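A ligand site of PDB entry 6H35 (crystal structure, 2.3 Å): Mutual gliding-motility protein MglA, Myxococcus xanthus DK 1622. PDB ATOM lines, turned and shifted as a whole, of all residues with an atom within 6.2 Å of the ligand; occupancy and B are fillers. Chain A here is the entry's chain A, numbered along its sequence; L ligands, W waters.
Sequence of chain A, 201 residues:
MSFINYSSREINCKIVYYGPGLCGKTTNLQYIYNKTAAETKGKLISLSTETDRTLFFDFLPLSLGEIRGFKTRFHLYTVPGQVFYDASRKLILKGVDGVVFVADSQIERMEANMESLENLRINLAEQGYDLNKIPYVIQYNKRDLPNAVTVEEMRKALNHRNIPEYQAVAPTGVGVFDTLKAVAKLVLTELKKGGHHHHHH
NH2 of Arg 53 is in salt-bridge range of O6 of the ligand, 2.6 Å away. The backbone NH of Thr 26 lies within hydrogen-bond range of an oxygen (O3) of the ligand (2.8 Å). OG1 of Thr 26 is in hydrogen-bond range of O3 of the ligand (2.7 Å). The side-chain carboxylate of Asp 144 sits at hydrogen-bond distance from a nitrogen (N4) of the ligand, at 2.7 Å. An oxygen (O5) of the ligand is in hydrogen-bond range of the backbone NH (N) of Thr 27, 2.9 Å away. The side-chain hydroxyl (OG1) of Thr 27 lies within hydrogen-bond range of an oxygen (O5) of the ligand (2.7 Å). N of Lys 25 lies within hydrogen-bond range of O1 of the ligand (2.9 Å). O1 of the ligand lies within salt-bridge range of NZ of Lys 25 (3.0 Å). An oxygen (O2) of the ligand lies within hydrogen-bond range of the backbone NH (N) of Leu 22 (2.9 Å). O1 of the ligand lies within hydrogen-bond range of N of Gly 24, 3.0 Å away. The side-chain amide nitrogen (ND2) of Asn 141 lies within hydrogen-bond range of a nitrogen (N2) of the ligand (3.0 Å). O11 of the ligand sits at hydrogen-bond distance from N of Lys 142 (3.2 Å). N of Cys 23 lies within hydrogen-bond range of O1 of the ligand (3.2 Å). The side-chain sulfur (SG) of Cys 23 lies within hydrogen-bond range of an oxygen (O1) of the ligand. N of Ala 170 is in hydrogen-bond range of O11 of the ligand (3.3 Å).
Water W1 lies within hydrogen-bond range of O2 of the ligand (2.6 Å) and NZ of Lys 25 (2.9 Å). Water W2 lies within hydrogen-bond range of an oxygen (O6) of the ligand and the guanidinium group of Arg 53.
NH2 of Arg 53 is in hydrogen-bond range of OG1 of Thr 26 (3.2 Å). The side-chain amino group (NZ) of Lys 25 sits at hydrogen-bond distance from the backbone carbonyl oxygen (O) of Pro 20 (3.1 Å). The side-chain amino group (NZ) of Lys 142 sits at hydrogen-bond distance from the backbone carbonyl oxygen (O) of Leu 22 (2.7 Å). The backbone carbonyl oxygen of Gly 24 lies within hydrogen-bond range of the side-chain amide nitrogen of Asn 28. The side-chain amide nitrogen (ND2) of Asn 141 is in hydrogen-bond range of the backbone carbonyl oxygen (O) of Cys 23, 2.9 Å away. The side-chain amide oxygen (OD1) of Asn 141 sits at hydrogen-bond distance from the backbone NH (N) of Ala 170. The backbone NH of Lys 142 is in hydrogen-bond range of the backbone carbonyl oxygen of Ala 168. SG of Cys 23 sits at hydrogen-bond distance from O of Pro 20.
Merely in contact with the ligand: Pro 171, Leu 145, Val 169 and Pro 20. 15 residues have an atom within 4 Å of the ligand: Pro 20, Leu 22, Cys 23, Gly 24, Lys 25, Thr 26, Thr 27, Arg 53, Asn 141, Lys 142, Asp 144, Leu 145, Val 169, Ala 170 and Pro 171. The nearest printed residue that does not touch the ligand is Gly 21 (4.02 Å).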
ATOM      1  N   GLY A  19       2.632  17.137   4.793  1.00  0.00           N
ATOM      2  CA  GLY A  19       1.586  16.486   5.550  1.00  0.00           C
ATOM      3  C   GLY A  19       0.319  16.313   4.744  1.00  0.00           C
ATOM      4  O   GLY A  19       0.169  16.881   3.656  1.00  0.00           O
ATOM      5  N   PRO A  20      -0.624  15.539   5.273  1.00  0.00           N
ATOM      6  CA  PRO A  20      -1.857  15.272   4.547  1.00  0.00           C
ATOM      7  C   PRO A  20      -2.740  16.510   4.503  1.00  0.00           C
ATOM      8  O   PRO A  20      -2.548  17.481   5.233  1.00  0.00           O
ATOM      9  CB  PRO A  20      -2.510  14.156   5.352  1.00  0.00           C
ATOM     10  CG  PRO A  20      -2.049  14.404   6.747  1.00  0.00           C
ATOM     11  CD  PRO A  20      -0.640  14.940   6.626  1.00  0.00           C
ATOM     12  N   GLY A  21      -3.752  16.457   3.623  1.00  0.00           N
ATOM     13  CA  GLY A  21      -4.697  17.533   3.495  1.00  0.00           C
ATOM     14  C   GLY A  21      -5.368  17.920   4.800  1.00  0.00           C
ATOM     15  O   GLY A  21      -5.800  17.059   5.569  1.00  0.00           O
ATOM     16  N   LEU A  22      -5.416  19.229   5.058  1.00  0.00           N
ATOM     17  CA  LEU A  22      -6.099  19.835   6.195  1.00  0.00           C
ATOM     18  C   LEU A  22      -5.417  19.516   7.524  1.00  0.00           C
ATOM     19  O   LEU A  22      -6.070  19.553   8.573  1.00  0.00           O
ATOM     20  CB  LEU A  22      -7.573  19.414   6.268  1.00  0.00           C
ATOM     21  CG  LEU A  22      -8.411  19.753   5.029  1.00  0.00           C
ATOM     22  CD1 LEU A  22      -9.684  18.917   5.026  1.00  0.00           C
ATOM     23  CD2 LEU A  22      -8.740  21.232   5.007  1.00  0.00           C
ATOM     24  N   CYS A  23      -4.117  19.238   7.520  1.00  0.00           N
ATOM     25  CA  CYS A  23      -3.436  18.943   8.763  1.00  0.00           C
ATOM     26  C   CYS A  23      -2.931  20.199   9.465  1.00  0.00           C
ATOM     27  O   CYS A  23      -2.735  20.180  10.689  1.00  0.00           O
ATOM     28  CB  CYS A  23      -2.281  17.975   8.520  1.00  0.00           C
ATOM     29  SG  CYS A  23      -0.953  18.716   7.576  1.00  0.00           S
ATOM     30  N   GLY A  24      -2.716  21.280   8.724  1.00  0.00           N
ATOM     31  CA  GLY A  24      -2.331  22.542   9.336  1.00  0.00           C
ATOM     32  C   GLY A  24      -1.079  23.200   8.773  1.00  0.00           C
ATOM     33  O   GLY A  24      -0.405  23.951   9.472  1.00  0.00           O
ATOM     34  N   LYS A  25      -0.759  22.935   7.499  1.00  0.00           N
ATOM     35  CA  LYS A  25       0.430  23.534   6.907  1.00  0.00           C
ATOM     36  C   LYS A  25       0.212  25.015   6.635  1.00  0.00           C
ATOM     37  O   LYS A  25       1.024  25.865   7.030  1.00  0.00           O
ATOM     38  CB  LYS A  25       0.809  22.787   5.629  1.00  0.00           C
ATOM     39  CG  LYS A  25       0.878  21.276   5.803  1.00  0.00           C
ATOM     40  CD  LYS A  25       1.367  20.574   4.536  1.00  0.00           C
ATOM     41  CE  LYS A  25       0.305  20.545   3.446  1.00  0.00           C
ATOM     42  NZ  LYS A  25      -0.859  19.692   3.827  1.00  0.00           N
ATOM     43  N   THR A  26      -0.883  25.334   5.949  1.00  0.00           N
ATOM     44  CA  THR A  26      -1.227  26.726   5.686  1.00  0.00           C
ATOM     45  C   THR A  26      -1.271  27.526   6.979  1.00  0.00           C
ATOM     46  O   THR A  26      -0.805  28.667   7.025  1.00  0.00           O
ATOM     47  CB  THR A  26      -2.573  26.819   4.965  1.00  0.00           C
ATOM     48  OG1 THR A  26      -2.489  26.122   3.708  1.00  0.00           O
ATOM     49  CG2 THR A  26      -2.939  28.263   4.698  1.00  0.00           C
ATOM     50  N   THR A  27      -1.826  26.946   8.038  1.00  0.00           N
ATOM     51  CA  THR A  27      -1.935  27.656   9.308  1.00  0.00           C
ATOM     52  C   THR A  27      -0.567  27.944   9.899  1.00  0.00           C
ATOM     53  O   THR A  27      -0.321  29.050  10.410  1.00  0.00           O
ATOM     54  CB  THR A  27      -2.793  26.847  10.280  1.00  0.00           C
ATOM     55  OG1 THR A  27      -4.048  26.548   9.657  1.00  0.00           O
ATOM     56  CG2 THR A  27      -3.047  27.629  11.548  1.00  0.00           C
ATOM     57  N   ASN A  28       0.333  26.966   9.855  1.00  0.00           N
ATOM     58  CA  ASN A  28       1.709  27.186  10.322  1.00  0.00           C
ATOM     59  C   ASN A  28       2.355  28.341   9.574  1.00  0.00           C
ATOM     60  O   ASN A  28       2.928  29.259  10.193  1.00  0.00           O
ATOM     61  CB  ASN A  28       2.534  25.906  10.147  1.00  0.00           C
ATOM     62  CG  ASN A  28       2.431  24.968  11.337  1.00  0.00           C
ATOM     63  OD1 ASN A  28       3.305  24.941  12.196  1.00  0.00           O
ATOM     64  ND2 ASN A  28       1.353  24.184  11.378  1.00  0.00           N
ATOM     65  N   GLN A  30       0.957  30.739   7.840  1.00  0.00           N
ATOM     66  CA  GLN A  30       0.237  31.983   8.093  1.00  0.00           C
ATOM     67  C   GLN A  30       0.653  32.590   9.427  1.00  0.00           C
ATOM     68  O   GLN A  30       0.935  33.798   9.521  1.00  0.00           O
ATOM     69  CB  GLN A  30      -1.268  31.740   8.070  1.00  0.00           C
ATOM     70  CG  GLN A  30      -1.924  31.906   6.709  1.00  0.00           C
ATOM     71  CD  GLN A  30      -3.400  31.548   6.721  1.00  0.00           C
ATOM     72  OE1 GLN A  30      -4.167  32.025   5.879  1.00  0.00           O
ATOM     73  NE2 GLN A  30      -3.796  30.716   7.664  1.00  0.00           N
ATOM     74  N   ARG A  53      -3.977  24.137  -3.249  1.00  0.00           N
ATOM     75  CA  ARG A  53      -3.225  25.376  -3.133  1.00  0.00           C
ATOM     76  C   ARG A  53      -1.823  25.075  -2.617  1.00  0.00           C
ATOM     77  O   ARG A  53      -1.543  24.001  -2.083  1.00  0.00           O
ATOM     78  CB  ARG A  53      -3.920  26.380  -2.205  1.00  0.00           C
ATOM     79  CG  ARG A  53      -3.843  26.004  -0.741  1.00  0.00           C
ATOM     80  CD  ARG A  53      -4.817  26.805   0.113  1.00  0.00           C
ATOM     81  NE  ARG A  53      -4.885  26.285   1.474  1.00  0.00           N
ATOM     82  CZ  ARG A  53      -5.637  26.811   2.442  1.00  0.00           C
ATOM     83  NH1 ARG A  53      -6.377  27.884   2.200  1.00  0.00           N
ATOM     84  NH2 ARG A  53      -5.636  26.268   3.649  1.00  0.00           N
ATOM     85  N   THR A  78       4.552  25.372   1.659  1.00  0.00           N
ATOM     86  CA  THR A  78       3.666  24.247   1.904  1.00  0.00           C
ATOM     87  C   THR A  78       3.636  23.367   0.659  1.00  0.00           C
ATOM     88  O   THR A  78       4.293  23.642  -0.339  1.00  0.00           O
ATOM     89  CB  THR A  78       2.251  24.699   2.275  1.00  0.00           C
ATOM     90  OG1 THR A  78       1.592  25.217   1.115  1.00  0.00           O
ATOM     91  CG2 THR A  78       2.296  25.756   3.363  1.00  0.00           C
ATOM     92  N   VAL A  79       2.828  22.319   0.720  1.00  0.00           N
ATOM     93  CA  VAL A  79       2.771  21.328  -0.346  1.00  0.00           C
ATOM     94  C   VAL A  79       1.300  21.098  -0.657  1.00  0.00           C
ATOM     95  O   VAL A  79       0.458  21.223   0.251  1.00  0.00           O
ATOM     96  CB  VAL A  79       3.531  20.055   0.060  1.00  0.00           C
ATOM     97  CG1 VAL A  79       2.589  18.888   0.271  1.00  0.00           C
ATOM     98  CG2 VAL A  79       4.618  19.716  -0.935  1.00  0.00           C
ATOM     99  N   GLY A  81      -2.214  19.066  -1.314  1.00  0.00           N
ATOM    100  CA  GLY A  81      -2.727  17.933  -0.566  1.00  0.00           C
ATOM    101  C   GLY A  81      -3.541  16.920  -1.347  1.00  0.00           C
ATOM    102  O   GLY A  81      -3.797  15.818  -0.844  1.00  0.00           O
ATOM    103  N   ASN A 141       0.164  18.300  15.431  1.00  0.00           N
ATOM    104  CA  ASN A 141      -0.714  19.455  15.461  1.00  0.00           C
ATOM    105  C   ASN A 141      -2.105  19.054  15.928  1.00  0.00           C
ATOM    106  O   ASN A 141      -2.458  17.873  15.958  1.00  0.00           O
ATOM    107  CB  ASN A 141      -0.771  20.098  14.074  1.00  0.00           C
ATOM    108  CG  ASN A 141      -1.367  21.488  14.091  1.00  0.00           C
ATOM    109  OD1 ASN A 141      -1.139  22.261  15.022  1.00  0.00           O
ATOM    110  ND2 ASN A 141      -2.129  21.813  13.056  1.00  0.00           N
ATOM    111  N   LYS A 142      -2.894  20.058  16.307  1.00  0.00           N
ATOM    112  CA  LYS A 142      -4.288  19.877  16.758  1.00  0.00           C
ATOM    113  C   LYS A 142      -4.366  19.144  18.095  1.00  0.00           C
ATOM    114  O   LYS A 142      -5.225  18.287  18.300  1.00  0.00           O
ATOM    115  CB  LYS A 142      -5.127  19.159  15.695  1.00  0.00           C
ATOM    116  CG  LYS A 142      -4.959  19.716  14.296  1.00  0.00           C
ATOM    117  CD  LYS A 142      -6.149  19.392  13.415  1.00  0.00           C
ATOM    118  CE  LYS A 142      -5.892  19.797  11.961  1.00  0.00           C
ATOM    119  NZ  LYS A 142      -7.040  19.473  11.061  1.00  0.00           N
ATOM    120  N   ARG A 143      -3.485  19.501  19.034  1.00  0.00           N
ATOM    121  CA  ARG A 143      -3.547  18.905  20.366  1.00  0.00           C
ATOM    122  C   ARG A 143      -4.742  19.405  21.160  1.00  0.00           C
ATOM    123  O   ARG A 143      -5.053  18.831  22.208  1.00  0.00           O
ATOM    124  CB  ARG A 143      -2.258  19.207  21.147  1.00  0.00           C
ATOM    125  CG  ARG A 143      -0.982  18.786  20.447  1.00  0.00           C
ATOM    126  CD  ARG A 143      -1.035  17.322  20.028  1.00  0.00           C
ATOM    127  NE  ARG A 143      -1.271  16.425  21.156  1.00  0.00           N
ATOM    128  CZ  ARG A 143      -1.409  15.105  21.031  1.00  0.00           C
ATOM    129  NH1 ARG A 143      -1.355  14.546  19.830  1.00  0.00           N
ATOM    130  NH2 ARG A 143      -1.622  14.350  22.099  1.00  0.00           N
ATOM    131  N   ASP A 144      -5.411  20.458  20.689  1.00  0.00           N
ATOM    132  CA  ASP A 144      -6.565  20.975  21.399  1.00  0.00           C
ATOM    133  C   ASP A 144      -7.797  20.088  21.220  1.00  0.00           C
ATOM    134  O   ASP A 144      -8.714  20.145  22.041  1.00  0.00           O
ATOM    135  CB  ASP A 144      -6.877  22.385  20.909  1.00  0.00           C
ATOM    136  CG  ASP A 144      -7.082  22.439  19.412  1.00  0.00           C
ATOM    137  OD1 ASP A 144      -6.201  21.961  18.668  1.00  0.00           O
ATOM    138  OD2 ASP A 144      -8.150  22.918  18.963  1.00  0.00           O
ATOM    139  N   LEU A 145      -7.825  19.279  20.170  1.00  0.00           N
ATOM    140  CA  LEU A 145      -9.046  18.558  19.827  1.00  0.00           C
ATOM    141  C   LEU A 145      -9.244  17.362  20.759  1.00  0.00           C
ATOM    142  O   LEU A 145      -8.271  16.744  21.209  1.00  0.00           O
ATOM    143  CB  LEU A 145      -8.999  18.105  18.372  1.00  0.00           C
ATOM    144  CG  LEU A 145      -9.100  19.234  17.338  1.00  0.00           C
ATOM    145  CD1 LEU A 145      -9.147  18.685  15.918  1.00  0.00           C
ATOM    146  CD2 LEU A 145     -10.315  20.111  17.608  1.00  0.00           C
ATOM    147  N   ALA A 168       1.657  21.081  18.924  1.00  0.00           N
ATOM    148  CA  ALA A 168       1.255  22.385  18.439  1.00  0.00           C
ATOM    149  C   ALA A 168      -0.259  22.537  18.426  1.00  0.00           C
ATOM    150  O   ALA A 168      -1.005  21.566  18.275  1.00  0.00           O
ATOM    151  CB  ALA A 168       1.787  22.652  17.024  1.00  0.00           C
ATOM    152  N   VAL A 169      -0.691  23.783  18.588  1.00  0.00           N
ATOM    153  CA  VAL A 169      -2.044  24.217  18.236  1.00  0.00           C
ATOM    154  C   VAL A 169      -1.845  25.397  17.286  1.00  0.00           C
ATOM    155  O   VAL A 169      -1.784  26.559  17.712  1.00  0.00           O
ATOM    156  CB  VAL A 169      -2.881  24.606  19.450  1.00  0.00           C
ATOM    157  CG1 VAL A 169      -4.332  24.859  19.056  1.00  0.00           C
ATOM    158  CG2 VAL A 169      -2.803  23.517  20.514  1.00  0.00           C
ATOM    159  N   ALA A 170      -1.700  25.089  15.994  1.00  0.00           N
ATOM    160  CA  ALA A 170      -1.201  26.077  15.045  1.00  0.00           C
ATOM    161  C   ALA A 170      -2.024  27.360  14.971  1.00  0.00           C
ATOM    162  O   ALA A 170      -1.401  28.440  14.902  1.00  0.00           O
ATOM    163  CB  ALA A 170      -1.091  25.427  13.661  1.00  0.00           C
ATOM    164  N   PRO A 171      -3.366  27.346  14.980  1.00  0.00           N
ATOM    165  CA  PRO A 171      -4.085  28.623  14.875  1.00  0.00           C
ATOM    166  C   PRO A 171      -3.739  29.604  15.986  1.00  0.00           C
ATOM    167  O   PRO A 171      -3.657  30.810  15.739  1.00  0.00           O
ATOM    168  CB  PRO A 171      -5.561  28.200  14.939  1.00  0.00           C
ATOM    169  CG  PRO A 171      -5.568  26.810  14.446  1.00  0.00           C
ATOM    170  CD  PRO A 171      -4.299  26.212  14.977  1.00  0.00           C
HETATM  171  P1  LIG L   1      -3.503  22.359   5.243  1.00  0.00           P
HETATM  172  O1  LIG L   1      -2.462  21.400   5.777  1.00  0.00           O
HETATM  173  O2  LIG L   1      -4.151  21.679   4.072  1.00  0.00           O
HETATM  174  O3  LIG L   1      -2.851  23.657   4.811  1.00  0.00           O
HETATM  175  O4  LIG L   1      -4.588  22.657   6.389  1.00  0.00           O
HETATM  176  P2  LIG L   1      -4.971  24.116   6.950  1.00  0.00           P
HETATM  177  O5  LIG L   1      -3.790  24.884   7.501  1.00  0.00           O
HETATM  178  O6  LIG L   1      -5.705  24.920   5.913  1.00  0.00           O
HETATM  179  O7  LIG L   1      -5.978  23.723   8.133  1.00  0.00           O
HETATM  180  C1  LIG L   1      -7.191  23.067   7.798  1.00  0.00           C
HETATM  181  C2  LIG L   1      -8.217  23.398   8.864  1.00  0.00           C
HETATM  182  O8  LIG L   1      -7.773  22.893  10.118  1.00  0.00           O
HETATM  183  C3  LIG L   1      -8.346  24.903   9.014  1.00  0.00           C
HETATM  184  O9  LIG L   1      -9.734  25.195   9.055  1.00  0.00           O
HETATM  185  C4  LIG L   1      -7.705  25.227  10.349  1.00  0.00           C
HETATM  186  O10 LIG L   1      -8.405  26.269  11.024  1.00  0.00           O
HETATM  187  C5  LIG L   1      -7.808  23.924  11.103  1.00  0.00           C
HETATM  188  N1  LIG L   1      -6.678  23.731  12.040  1.00  0.00           N
HETATM  189  C6  LIG L   1      -5.369  23.760  11.725  1.00  0.00           C
HETATM  190  N2  LIG L   1      -4.601  23.526  12.826  1.00  0.00           N
HETATM  191  C7  LIG L   1      -5.445  23.316  13.862  1.00  0.00           C
HETATM  192  C8  LIG L   1      -5.301  23.019  15.308  1.00  0.00           C
HETATM  193  O11 LIG L   1      -4.183  22.895  15.833  1.00  0.00           O
HETATM  194  N3  LIG L   1      -6.420  22.879  16.027  1.00  0.00           N
HETATM  195  C9  LIG L   1      -7.645  23.013  15.492  1.00  0.00           C
HETATM  196  N4  LIG L   1      -8.735  22.860  16.300  1.00  0.00           N
HETATM  197  N5  LIG L   1      -7.847  23.289  14.174  1.00  0.00           N
HETATM  198  C10 LIG L   1      -6.801  23.451  13.332  1.00  0.00           C
HETATM  199  O   HOH W   1      -3.078  20.426   2.073  1.00  0.00           O
HETATM  200  O   HOH W   2      -6.359  27.639   6.477  1.00  0.00           O
HETATM  201  O   HOH W   3     -10.687  24.262   5.930  1.00  0.00           O
HETATM  202  O   HOH W   4     -10.035  27.131  13.151  1.00  0.00           O
